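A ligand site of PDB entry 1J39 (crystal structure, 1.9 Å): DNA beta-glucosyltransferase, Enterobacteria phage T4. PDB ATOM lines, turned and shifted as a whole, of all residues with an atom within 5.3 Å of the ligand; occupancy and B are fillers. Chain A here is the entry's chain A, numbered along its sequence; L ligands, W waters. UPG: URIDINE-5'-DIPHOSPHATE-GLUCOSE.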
ATOM      1  N   VAL A  18      25.366  29.043  -5.219  1.00  0.00           N
ATOM      2  CA  VAL A  18      24.376  28.130  -5.788  1.00  0.00           C
ATOM      3  C   VAL A  18      24.620  27.839  -7.264  1.00  0.00           C
ATOM      4  O   VAL A  18      24.623  26.683  -7.687  1.00  0.00           O
ATOM      5  CB  VAL A  18      22.936  28.676  -5.603  1.00  0.00           C
ATOM      6  CG1 VAL A  18      21.935  27.752  -6.283  1.00  0.00           C
ATOM      7  CG2 VAL A  18      22.623  28.803  -4.118  1.00  0.00           C
ATOM      8  N   GLU A  22      25.823  24.243  -8.379  1.00  0.00           N
ATOM      9  CA  GLU A  22      24.923  23.461  -9.224  1.00  0.00           C
ATOM     10  C   GLU A  22      25.604  23.083 -10.529  1.00  0.00           C
ATOM     11  O   GLU A  22      25.368  22.001 -11.066  1.00  0.00           O
ATOM     12  CB  GLU A  22      23.611  24.233  -9.512  1.00  0.00           C
ATOM     13  CG  GLU A  22      22.760  23.619 -10.650  1.00  0.00           C
ATOM     14  CD  GLU A  22      21.367  24.248 -10.791  1.00  0.00           C
ATOM     15  OE1 GLU A  22      20.443  23.821 -10.069  1.00  0.00           O
ATOM     16  OE2 GLU A  22      21.199  25.156 -11.628  1.00  0.00           O
ATOM     17  N   THR A  99      16.382  26.282 -15.374  1.00  0.00           N
ATOM     18  CA  THR A  99      16.118  25.839 -13.996  1.00  0.00           C
ATOM     19  C   THR A  99      15.552  26.933 -13.078  1.00  0.00           C
ATOM     20  O   THR A  99      15.133  26.647 -11.957  1.00  0.00           O
ATOM     21  CB  THR A  99      17.398  25.309 -13.349  1.00  0.00           C
ATOM     22  OG1 THR A  99      18.375  26.362 -13.327  1.00  0.00           O
ATOM     23  CG2 THR A  99      17.951  24.124 -14.150  1.00  0.00           C
ATOM     24  N   ASP A 100      15.546  28.166 -13.558  1.00  0.00           N
ATOM     25  CA  ASP A 100      15.039  29.292 -12.779  1.00  0.00           C
ATOM     26  C   ASP A 100      14.225  30.188 -13.715  1.00  0.00           C
ATOM     27  O   ASP A 100      14.761  30.760 -14.660  1.00  0.00           O
ATOM     28  CB  ASP A 100      16.195  30.079 -12.166  1.00  0.00           C
ATOM     29  CG  ASP A 100      15.738  31.091 -11.132  1.00  0.00           C
ATOM     30  OD1 ASP A 100      14.750  31.797 -11.389  1.00  0.00           O
ATOM     31  OD2 ASP A 100      16.371  31.181 -10.065  1.00  0.00           O
ATOM     32  N   GLN A 137      12.797  22.867 -16.766  1.00  0.00           N
ATOM     33  CA  GLN A 137      12.669  22.085 -15.550  1.00  0.00           C
ATOM     34  C   GLN A 137      11.175  22.006 -15.234  1.00  0.00           C
ATOM     35  O   GLN A 137      10.714  21.080 -14.574  1.00  0.00           O
ATOM     36  CB  GLN A 137      13.425  22.764 -14.415  1.00  0.00           C
ATOM     37  CG  GLN A 137      13.451  21.981 -13.106  1.00  0.00           C
ATOM     38  CD  GLN A 137      14.402  22.599 -12.101  1.00  0.00           C
ATOM     39  OE1 GLN A 137      15.582  22.802 -12.382  1.00  0.00           O
ATOM     40  NE2 GLN A 137      13.885  22.907 -10.909  1.00  0.00           N
ATOM     41  N   GLU A 163      16.268  19.109 -11.886  1.00  0.00           N
ATOM     42  CA  GLU A 163      16.526  19.159 -10.441  1.00  0.00           C
ATOM     43  C   GLU A 163      16.682  17.829  -9.699  1.00  0.00           C
ATOM     44  O   GLU A 163      17.115  17.814  -8.548  1.00  0.00           O
ATOM     45  CB  GLU A 163      15.470  20.039  -9.753  1.00  0.00           C
ATOM     46  CG  GLU A 163      14.217  19.341  -9.223  1.00  0.00           C
ATOM     47  CD  GLU A 163      13.398  18.625 -10.280  1.00  0.00           C
ATOM     48  OE1 GLU A 163      13.376  19.079 -11.449  1.00  0.00           O
ATOM     49  OE2 GLU A 163      12.765  17.599  -9.936  1.00  0.00           O
ATOM     50  N   TYR A 165      18.870  15.799 -10.151  1.00  0.00           N
ATOM     51  CA  TYR A 165      20.291  15.424 -10.101  1.00  0.00           C
ATOM     52  C   TYR A 165      20.742  15.184  -8.667  1.00  0.00           C
ATOM     53  O   TYR A 165      21.655  14.403  -8.408  1.00  0.00           O
ATOM     54  CB  TYR A 165      21.154  16.506 -10.774  1.00  0.00           C
ATOM     55  CG  TYR A 165      21.198  17.852 -10.073  1.00  0.00           C
ATOM     56  CD1 TYR A 165      22.011  18.040  -8.951  1.00  0.00           C
ATOM     57  CD2 TYR A 165      20.459  18.928 -10.536  1.00  0.00           C
ATOM     58  CE1 TYR A 165      22.088  19.281  -8.319  1.00  0.00           C
ATOM     59  CE2 TYR A 165      20.526  20.177  -9.915  1.00  0.00           C
ATOM     60  CZ  TYR A 165      21.342  20.343  -8.811  1.00  0.00           C
ATOM     61  OH  TYR A 165      21.421  21.573  -8.197  1.00  0.00           O
ATOM     62  N   TYR A 186      13.224  27.002   6.753  1.00  0.00           N
ATOM     63  CA  TYR A 186      13.171  27.300   5.323  1.00  0.00           C
ATOM     64  C   TYR A 186      14.534  27.867   4.934  1.00  0.00           C
ATOM     65  O   TYR A 186      15.004  28.822   5.561  1.00  0.00           O
ATOM     66  CB  TYR A 186      12.092  28.337   5.020  1.00  0.00           C
ATOM     67  CG  TYR A 186      11.970  28.666   3.542  1.00  0.00           C
ATOM     68  CD1 TYR A 186      11.170  27.900   2.693  1.00  0.00           C
ATOM     69  CD2 TYR A 186      12.652  29.757   2.995  1.00  0.00           C
ATOM     70  CE1 TYR A 186      11.051  28.210   1.338  1.00  0.00           C
ATOM     71  CE2 TYR A 186      12.542  30.078   1.640  1.00  0.00           C
ATOM     72  CZ  TYR A 186      11.741  29.305   0.821  1.00  0.00           C
ATOM     73  OH  TYR A 186      11.609  29.625  -0.515  1.00  0.00           O
ATOM     74  N   GLY A 187      15.160  27.281   3.915  1.00  0.00           N
ATOM     75  CA  GLY A 187      16.463  27.749   3.480  1.00  0.00           C
ATOM     76  C   GLY A 187      16.412  28.279   2.061  1.00  0.00           C
ATOM     77  O   GLY A 187      16.015  27.564   1.147  1.00  0.00           O
ATOM     78  N   GLY A 188      16.817  29.527   1.882  1.00  0.00           N
ATOM     79  CA  GLY A 188      16.786  30.107   0.560  1.00  0.00           C
ATOM     80  C   GLY A 188      17.080  31.587   0.564  1.00  0.00           C
ATOM     81  O   GLY A 188      17.575  32.133   1.550  1.00  0.00           O
ATOM     82  N   SER A 189      16.768  32.248  -0.545  1.00  0.00           N
ATOM     83  CA  SER A 189      17.025  33.673  -0.670  1.00  0.00           C
ATOM     84  C   SER A 189      15.717  34.455  -0.747  1.00  0.00           C
ATOM     85  O   SER A 189      14.646  33.892  -0.950  1.00  0.00           O
ATOM     86  CB  SER A 189      17.866  33.935  -1.917  1.00  0.00           C
ATOM     87  OG  SER A 189      17.218  33.454  -3.072  1.00  0.00           O
ATOM     88  N   ARG A 191      15.024  36.493  -3.021  1.00  0.00           N
ATOM     89  CA  ARG A 191      14.657  36.539  -4.442  1.00  0.00           C
ATOM     90  C   ARG A 191      13.900  37.810  -4.852  1.00  0.00           C
ATOM     91  O   ARG A 191      12.798  37.736  -5.403  1.00  0.00           O
ATOM     92  CB  ARG A 191      13.848  35.303  -4.818  1.00  0.00           C
ATOM     93  CG  ARG A 191      14.681  34.022  -4.905  1.00  0.00           C
ATOM     94  CD  ARG A 191      13.813  32.802  -5.176  1.00  0.00           C
ATOM     95  NE  ARG A 191      13.201  32.820  -6.503  1.00  0.00           N
ATOM     96  CZ  ARG A 191      13.818  32.465  -7.633  1.00  0.00           C
ATOM     97  NH1 ARG A 191      15.081  32.058  -7.602  1.00  0.00           N
ATOM     98  NH2 ARG A 191      13.180  32.517  -8.783  1.00  0.00           N
ATOM     99  N   ARG A 195       8.523  36.522  -3.507  1.00  0.00           N
ATOM    100  CA  ARG A 195       7.751  35.579  -2.698  1.00  0.00           C
ATOM    101  C   ARG A 195       7.504  36.125  -1.304  1.00  0.00           C
ATOM    102  O   ARG A 195       7.213  35.366  -0.374  1.00  0.00           O
ATOM    103  CB  ARG A 195       8.491  34.252  -2.566  1.00  0.00           C
ATOM    104  CG  ARG A 195       8.665  33.519  -3.868  1.00  0.00           C
ATOM    105  CD  ARG A 195       9.642  32.371  -3.703  1.00  0.00           C
ATOM    106  NE  ARG A 195       9.812  31.642  -4.955  1.00  0.00           N
ATOM    107  CZ  ARG A 195      10.747  30.728  -5.167  1.00  0.00           C
ATOM    108  NH1 ARG A 195      11.607  30.421  -4.209  1.00  0.00           N
ATOM    109  NH2 ARG A 195      10.822  30.131  -6.347  1.00  0.00           N
ATOM    110  N   PHE A 213      17.135  30.201   6.870  1.00  0.00           N
ATOM    111  CA  PHE A 213      18.565  30.261   6.611  1.00  0.00           C
ATOM    112  C   PHE A 213      18.837  30.556   5.136  1.00  0.00           C
ATOM    113  O   PHE A 213      18.026  30.231   4.277  1.00  0.00           O
ATOM    114  CB  PHE A 213      19.291  28.972   7.061  1.00  0.00           C
ATOM    115  CG  PHE A 213      18.943  27.729   6.277  1.00  0.00           C
ATOM    116  CD1 PHE A 213      17.819  26.971   6.611  1.00  0.00           C
ATOM    117  CD2 PHE A 213      19.770  27.287   5.251  1.00  0.00           C
ATOM    118  CE1 PHE A 213      17.540  25.783   5.938  1.00  0.00           C
ATOM    119  CE2 PHE A 213      19.502  26.089   4.570  1.00  0.00           C
ATOM    120  CZ  PHE A 213      18.387  25.333   4.924  1.00  0.00           C
ATOM    121  N   GLY A 214      19.975  31.190   4.875  1.00  0.00           N
ATOM    122  CA  GLY A 214      20.316  31.540   3.511  1.00  0.00           C
ATOM    123  C   GLY A 214      20.640  33.019   3.386  1.00  0.00           C
ATOM    124  O   GLY A 214      21.038  33.649   4.368  1.00  0.00           O
ATOM    125  N   GLY A 236      22.825  32.615   8.661  1.00  0.00           N
ATOM    126  CA  GLY A 236      23.649  32.659   7.461  1.00  0.00           C
ATOM    127  C   GLY A 236      23.540  31.540   6.434  1.00  0.00           C
ATOM    128  O   GLY A 236      22.895  30.513   6.666  1.00  0.00           O
ATOM    129  N   LYS A 237      24.187  31.750   5.297  1.00  0.00           N
ATOM    130  CA  LYS A 237      24.192  30.783   4.204  1.00  0.00           C
ATOM    131  C   LYS A 237      25.098  29.616   4.535  1.00  0.00           C
ATOM    132  O   LYS A 237      26.114  29.786   5.212  1.00  0.00           O
ATOM    133  CB  LYS A 237      24.718  31.423   2.909  1.00  0.00           C
ATOM    134  CG  LYS A 237      23.943  32.613   2.404  1.00  0.00           C
ATOM    135  CD  LYS A 237      24.603  33.175   1.147  1.00  0.00           C
ATOM    136  CE  LYS A 237      26.016  33.656   1.423  1.00  0.00           C
ATOM    137  NZ  LYS A 237      26.661  34.241   0.213  1.00  0.00           N
ATOM    138  N   ILE A 238      24.746  28.430   4.049  1.00  0.00           N
ATOM    139  CA  ILE A 238      25.559  27.248   4.284  1.00  0.00           C
ATOM    140  C   ILE A 238      25.774  26.544   2.943  1.00  0.00           C
ATOM    141  O   ILE A 238      25.096  26.851   1.958  1.00  0.00           O
ATOM    142  CB  ILE A 238      24.878  26.268   5.275  1.00  0.00           C
ATOM    143  CG1 ILE A 238      23.580  25.735   4.689  1.00  0.00           C
ATOM    144  CG2 ILE A 238      24.623  26.978   6.603  1.00  0.00           C
ATOM    145  CD1 ILE A 238      22.911  24.695   5.565  1.00  0.00           C
ATOM    146  N   PRO A 239      26.730  25.606   2.886  1.00  0.00           N
ATOM    147  CA  PRO A 239      27.010  24.866   1.653  1.00  0.00           C
ATOM    148  C   PRO A 239      25.793  24.097   1.165  1.00  0.00           C
ATOM    149  O   PRO A 239      24.989  23.614   1.962  1.00  0.00           O
ATOM    150  CB  PRO A 239      28.145  23.923   2.073  1.00  0.00           C
ATOM    151  CG  PRO A 239      28.859  24.712   3.125  1.00  0.00           C
ATOM    152  CD  PRO A 239      27.707  25.264   3.936  1.00  0.00           C
ATOM    153  N   MET A 240      25.653  23.975  -0.154  1.00  0.00           N
ATOM    154  CA  MET A 240      24.530  23.243  -0.739  1.00  0.00           C
ATOM    155  C   MET A 240      24.458  21.816  -0.227  1.00  0.00           C
ATOM    156  O   MET A 240      23.374  21.283   0.009  1.00  0.00           O
ATOM    157  CB  MET A 240      24.650  23.191  -2.255  1.00  0.00           C
ATOM    158  CG  MET A 240      24.072  24.374  -2.986  1.00  0.00           C
ATOM    159  SD  MET A 240      24.107  24.070  -4.769  1.00  0.00           S
ATOM    160  CE  MET A 240      22.896  22.768  -4.928  1.00  0.00           C
ATOM    161  N   VAL A 243      22.454  21.448   3.106  1.00  0.00           N
ATOM    162  CA  VAL A 243      21.050  21.858   3.206  1.00  0.00           C
ATOM    163  C   VAL A 243      20.117  20.817   3.830  1.00  0.00           C
ATOM    164  O   VAL A 243      19.328  21.149   4.717  1.00  0.00           O
ATOM    165  CB  VAL A 243      20.504  22.276   1.809  1.00  0.00           C
ATOM    166  CG1 VAL A 243      19.010  22.567   1.882  1.00  0.00           C
ATOM    167  CG2 VAL A 243      21.251  23.519   1.324  1.00  0.00           C
ATOM    168  N   TYR A 261       5.808  29.019 -10.979  1.00  0.00           N
ATOM    169  CA  TYR A 261       6.443  27.800 -10.462  1.00  0.00           C
ATOM    170  C   TYR A 261       5.324  26.823 -10.109  1.00  0.00           C
ATOM    171  O   TYR A 261       5.447  25.613 -10.326  1.00  0.00           O
ATOM    172  CB  TYR A 261       7.259  28.082  -9.197  1.00  0.00           C
ATOM    173  CG  TYR A 261       8.656  28.604  -9.448  1.00  0.00           C
ATOM    174  CD1 TYR A 261       8.882  29.949  -9.760  1.00  0.00           C
ATOM    175  CD2 TYR A 261       9.751  27.744  -9.411  1.00  0.00           C
ATOM    176  CE1 TYR A 261      10.164  30.411 -10.036  1.00  0.00           C
ATOM    177  CE2 TYR A 261      11.034  28.205  -9.696  1.00  0.00           C
ATOM    178  CZ  TYR A 261      11.240  29.538 -10.008  1.00  0.00           C
ATOM    179  OH  TYR A 261      12.495  29.986 -10.305  1.00  0.00           O
ATOM    180  N   PHE A 265       6.977  23.776 -11.912  1.00  0.00           N
ATOM    181  CA  PHE A 265       8.323  23.381 -11.493  1.00  0.00           C
ATOM    182  C   PHE A 265       8.355  22.554 -10.221  1.00  0.00           C
ATOM    183  O   PHE A 265       7.580  22.790  -9.293  1.00  0.00           O
ATOM    184  CB  PHE A 265       9.175  24.615 -11.164  1.00  0.00           C
ATOM    185  CG  PHE A 265       9.916  25.211 -12.328  1.00  0.00           C
ATOM    186  CD1 PHE A 265       9.234  25.707 -13.440  1.00  0.00           C
ATOM    187  CD2 PHE A 265      11.302  25.326 -12.283  1.00  0.00           C
ATOM    188  CE1 PHE A 265       9.935  26.321 -14.477  1.00  0.00           C
ATOM    189  CE2 PHE A 265      12.003  25.941 -13.320  1.00  0.00           C
ATOM    190  CZ  PHE A 265      11.319  26.439 -14.413  1.00  0.00           C
ATOM    191  N   ILE A 266       9.248  21.570 -10.188  1.00  0.00           N
ATOM    192  CA  ILE A 266       9.498  20.834  -8.967  1.00  0.00           C
ATOM    193  C   ILE A 266      10.876  21.448  -8.755  1.00  0.00           C
ATOM    194  O   ILE A 266      11.691  21.477  -9.672  1.00  0.00           O
ATOM    195  CB  ILE A 266       9.632  19.315  -9.166  1.00  0.00           C
ATOM    196  CG1 ILE A 266       8.258  18.705  -9.438  1.00  0.00           C
ATOM    197  CG2 ILE A 266      10.222  18.687  -7.888  1.00  0.00           C
ATOM    198  CD1 ILE A 266       7.248  18.972  -8.340  1.00  0.00           C
ATOM    199  N   THR A 267      11.135  21.998  -7.565  1.00  0.00           N
ATOM    200  CA  THR A 267      12.417  22.640  -7.303  1.00  0.00           C
ATOM    201  C   THR A 267      13.351  21.749  -6.509  1.00  0.00           C
ATOM    202  O   THR A 267      12.932  20.747  -5.940  1.00  0.00           O
ATOM    203  CB  THR A 267      12.197  23.956  -6.518  1.00  0.00           C
ATOM    204  OG1 THR A 267      11.451  23.675  -5.322  1.00  0.00           O
ATOM    205  CG2 THR A 267      11.419  24.963  -7.370  1.00  0.00           C
ATOM    206  N   LEU A 268      14.630  22.116  -6.495  1.00  0.00           N
ATOM    207  CA  LEU A 268      15.641  21.335  -5.766  1.00  0.00           C
ATOM    208  C   LEU A 268      15.211  21.169  -4.314  1.00  0.00           C
ATOM    209  O   LEU A 268      15.387  20.099  -3.714  1.00  0.00           O
ATOM    210  CB  LEU A 268      17.002  22.023  -5.824  1.00  0.00           C
ATOM    211  CG  LEU A 268      18.151  21.242  -5.195  1.00  0.00           C
ATOM    212  CD1 LEU A 268      18.349  19.928  -5.941  1.00  0.00           C
ATOM    213  CD2 LEU A 268      19.430  22.069  -5.221  1.00  0.00           C
ATOM    214  N   ARG A 269      14.653  22.239  -3.766  1.00  0.00           N
ATOM    215  CA  ARG A 269      14.163  22.273  -2.397  1.00  0.00           C
ATOM    216  C   ARG A 269      13.232  21.102  -2.093  1.00  0.00           C
ATOM    217  O   ARG A 269      13.277  20.543  -0.994  1.00  0.00           O
ATOM    218  CB  ARG A 269      13.419  23.593  -2.176  1.00  0.00           C
ATOM    219  CG  ARG A 269      12.553  23.670  -0.940  1.00  0.00           C
ATOM    220  CD  ARG A 269      11.702  24.937  -1.004  1.00  0.00           C
ATOM    221  NE  ARG A 269      12.518  26.093  -1.376  1.00  0.00           N
ATOM    222  CZ  ARG A 269      13.508  26.569  -0.638  1.00  0.00           C
ATOM    223  NH1 ARG A 269      13.800  25.992   0.532  1.00  0.00           N
ATOM    224  NH2 ARG A 269      14.227  27.594  -1.065  1.00  0.00           N
ATOM    225  N   GLU A 272      15.524  18.236  -1.427  1.00  0.00           N
ATOM    226  CA  GLU A 272      16.360  18.480  -0.257  1.00  0.00           C
ATOM    227  C   GLU A 272      15.528  18.341   1.011  1.00  0.00           C
ATOM    228  O   GLU A 272      16.026  17.938   2.070  1.00  0.00           O
ATOM    229  CB  GLU A 272      16.943  19.885  -0.286  1.00  0.00           C
ATOM    230  CG  GLU A 272      17.721  20.221  -1.555  1.00  0.00           C
ATOM    231  CD  GLU A 272      18.180  21.660  -1.565  1.00  0.00           C
ATOM    232  OE1 GLU A 272      17.353  22.555  -1.303  1.00  0.00           O
ATOM    233  OE2 GLU A 272      19.369  21.902  -1.859  1.00  0.00           O
HETATM  234  N1  UPG L   1      20.768  27.037  -0.450  1.00  0.00           N
HETATM  235  C2  UPG L   1      22.098  26.908  -0.076  1.00  0.00           C
HETATM  236  N3  UPG L   1      22.416  27.463   1.128  1.00  0.00           N
HETATM  237  C4  UPG L   1      21.565  28.101   2.004  1.00  0.00           C
HETATM  238  C5  UPG L   1      20.212  28.192   1.561  1.00  0.00           C
HETATM  239  C6  UPG L   1      19.861  27.667   0.373  1.00  0.00           C
HETATM  240  O2  UPG L   1      22.921  26.343  -0.780  1.00  0.00           O
HETATM  241  O4  UPG L   1      22.011  28.551   3.066  1.00  0.00           O
HETATM  242  C1C UPG L   1      20.386  26.460  -1.737  1.00  0.00           C
HETATM  243  C2C UPG L   1      19.477  25.218  -1.667  1.00  0.00           C
HETATM  244  O2C UPG L   1      20.076  24.201  -2.429  1.00  0.00           O
HETATM  245  C3C UPG L   1      18.188  25.728  -2.313  1.00  0.00           C
HETATM  246  C4C UPG L   1      18.718  26.727  -3.316  1.00  0.00           C
HETATM  247  O4C UPG L   1      19.719  27.419  -2.536  1.00  0.00           O
HETATM  248  O3C UPG L   1      17.506  24.667  -2.956  1.00  0.00           O
HETATM  249  C5C UPG L   1      17.759  27.689  -3.977  1.00  0.00           C
HETATM  250  O5C UPG L   1      16.970  28.361  -3.008  1.00  0.00           O
HETATM  251  PA  UPG L   1      16.326  29.788  -3.333  1.00  0.00           P
HETATM  252  O1A UPG L   1      15.325  30.101  -2.278  1.00  0.00           O
HETATM  253  O2A UPG L   1      17.432  30.731  -3.603  1.00  0.00           O
HETATM  254  O3A UPG L   1      15.556  29.565  -4.751  1.00  0.00           O
HETATM  255  PB  UPG L   1      14.452  28.463  -5.211  1.00  0.00           P
HETATM  256  O1B UPG L   1      13.447  29.143  -6.062  1.00  0.00           O
HETATM  257  O2B UPG L   1      13.995  27.677  -4.030  1.00  0.00           O
HETATM  258  O3B UPG L   1      15.310  27.507  -6.150  1.00  0.00           O
HETATM  259  C1' UPG L   1      15.949  27.910  -7.365  1.00  0.00           C
HETATM  260  C2' UPG L   1      15.096  27.679  -8.597  1.00  0.00           C
HETATM  261  C3' UPG L   1      14.788  26.183  -8.671  1.00  0.00           C
HETATM  262  C4' UPG L   1      16.085  25.370  -8.703  1.00  0.00           C
HETATM  263  C5' UPG L   1      16.990  25.752  -7.510  1.00  0.00           C
HETATM  264  C6' UPG L   1      18.359  25.137  -7.624  1.00  0.00           C
HETATM  265  O2' UPG L   1      13.890  28.424  -8.502  1.00  0.00           O
HETATM  266  O3' UPG L   1      13.984  25.883  -9.813  1.00  0.00           O
HETATM  267  O4' UPG L   1      15.779  23.987  -8.635  1.00  0.00           O
HETATM  268  O5' UPG L   1      17.184  27.187  -7.469  1.00  0.00           O
HETATM  269  O6' UPG L   1      19.118  25.767  -8.648  1.00  0.00           O
HETATM  270  O   HOH W   1      17.314  32.120  -5.807  1.00  0.00           O
HETATM  271  O   HOH W   2      13.289  31.474  -1.747  1.00  0.00           O
HETATM  272  O   HOH W   3      17.438  22.802 -10.449  1.00  0.00           O
HETATM  273  O   HOH W   4      11.288  26.273  -4.102  1.00  0.00           O
HETATM  274  O   HOH W   5      18.622  27.733 -11.083  1.00  0.00           O
HETATM  275  O   HOH W   6      15.217  25.015  -4.519  1.00  0.00           O
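The side-chain carboxylate (OE1) of Glu 22 lies within hydrogen-bond range of the side-chain hydroxyl (OH) of Tyr 165, 3.1 Å away. OH of Tyr 261 sits at hydrogen-bond distance from NH2 of Arg 191 (3.0 Å). OH of Tyr 261 is in hydrogen-bond range of OD1 of Asp 100. The guanidinium group (NH1) of Arg 269 lies within hydrogen-bond range of the backbone carbonyl oxygen (O) of Gly 187 (2.8 Å). NE2 of Gln 137 is in hydrogen-bond range of O of Ile 266 (2.9 Å). N of Gly 188 sits at hydrogen-bond distance from O of Phe 213. The backbone NH of Gly 214 is in hydrogen-bond range of the backbone carbonyl oxygen of Gly 236 (3.5 Å). The side-chain carboxylate of Asp 100 lies within salt-bridge range of the guanidinium group of Arg 191 (2.9 Å).
OE2 of Glu 272 sits at hydrogen-bond distance from O2C of the ligand, 2.5 Å away. The backbone carbonyl oxygen of Thr 99 sits at hydrogen-bond distance from an oxygen (O3') of the ligand (2.5 Å). An oxygen (O6') of the ligand sits at hydrogen-bond distance from the side-chain carboxylate of Glu 22 (2.7 Å). The side-chain hydroxyl (OH) of Tyr 261 lies within hydrogen-bond range of an oxygen (O2') of the ligand, 2.8 Å away. The backbone NH (N) of Ser 189 lies within hydrogen-bond range of an oxygen (O1A) of the ligand (3.1 Å). The side-chain hydroxyl (OG) of Ser 189 is in hydrogen-bond range of an oxygen (O2A) of the ligand, 2.8 Å away. O1B of the ligand lies within salt-bridge range of NH2 of Arg 195, 2.8 Å away. An oxygen (O4) of the ligand is in hydrogen-bond range of the backbone NH (N) of Ile 238 (2.9 Å). The backbone carbonyl oxygen (O) of Ile 238 lies within hydrogen-bond range of a nitrogen (N3) of the ligand. O2B of the ligand lies within salt-bridge range of NH2 of Arg 269 (3.0 Å). An oxygen (O4') of the ligand lies within hydrogen-bond range of the backbone NH (N) of Leu 268, 3.1 Å away. The side-chain amide nitrogen of Gln 137 sits at hydrogen-bond distance from an oxygen (O4') of the ligand (3.2 Å). NH1 of Arg 191 lies within salt-bridge range of O1B of the ligand (3.7 Å).
Merely in contact with the ligand: Met 240, Gly 188, Lys 237, Phe 213, Gly 214, Val 18, Thr 267, Phe 265, Val 243 and Gly 187. Of the 28 residues printed, 21 come within 4 Å of the ligand. The nearest printed residue that does not touch the ligand is Asp 100 (4.01 Å).
Water W2 lies within hydrogen-bond range of an oxygen (O1A) of the ligand (2.5 Å), the side-chain hydroxyl of Tyr 186 (2.8 Å), the backbone carbonyl oxygen of Ser 189 (2.9 Å) and the guanidinium group of Arg 195 (3.2 Å). Water W1 lies within hydrogen-bond range of an oxygen (O2A) of the ligand, the guanidinium group (NH1) of Arg 191 and the side-chain hydroxyl (OG) of Ser 189. Water W3 lies within hydrogen-bond range of the side-chain amide oxygen of Gln 137, an oxygen (O4') of the ligand and the side-chain carboxylate of Glu 22. Water W6 bridges an oxygen (O3C) of the ligand and the backbone NH (N) of Arg 269. Water W4 lies within hydrogen-bond range of the side-chain hydroxyl (OG1) of Thr 267, the guanidinium group (NE) of Arg 269 and an oxygen (O2B) of the ligand. Water W5 lies within hydrogen-bond range of OG1 of Thr 99 (2.6 Å) and O6' of the ligand (3.2 Å).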
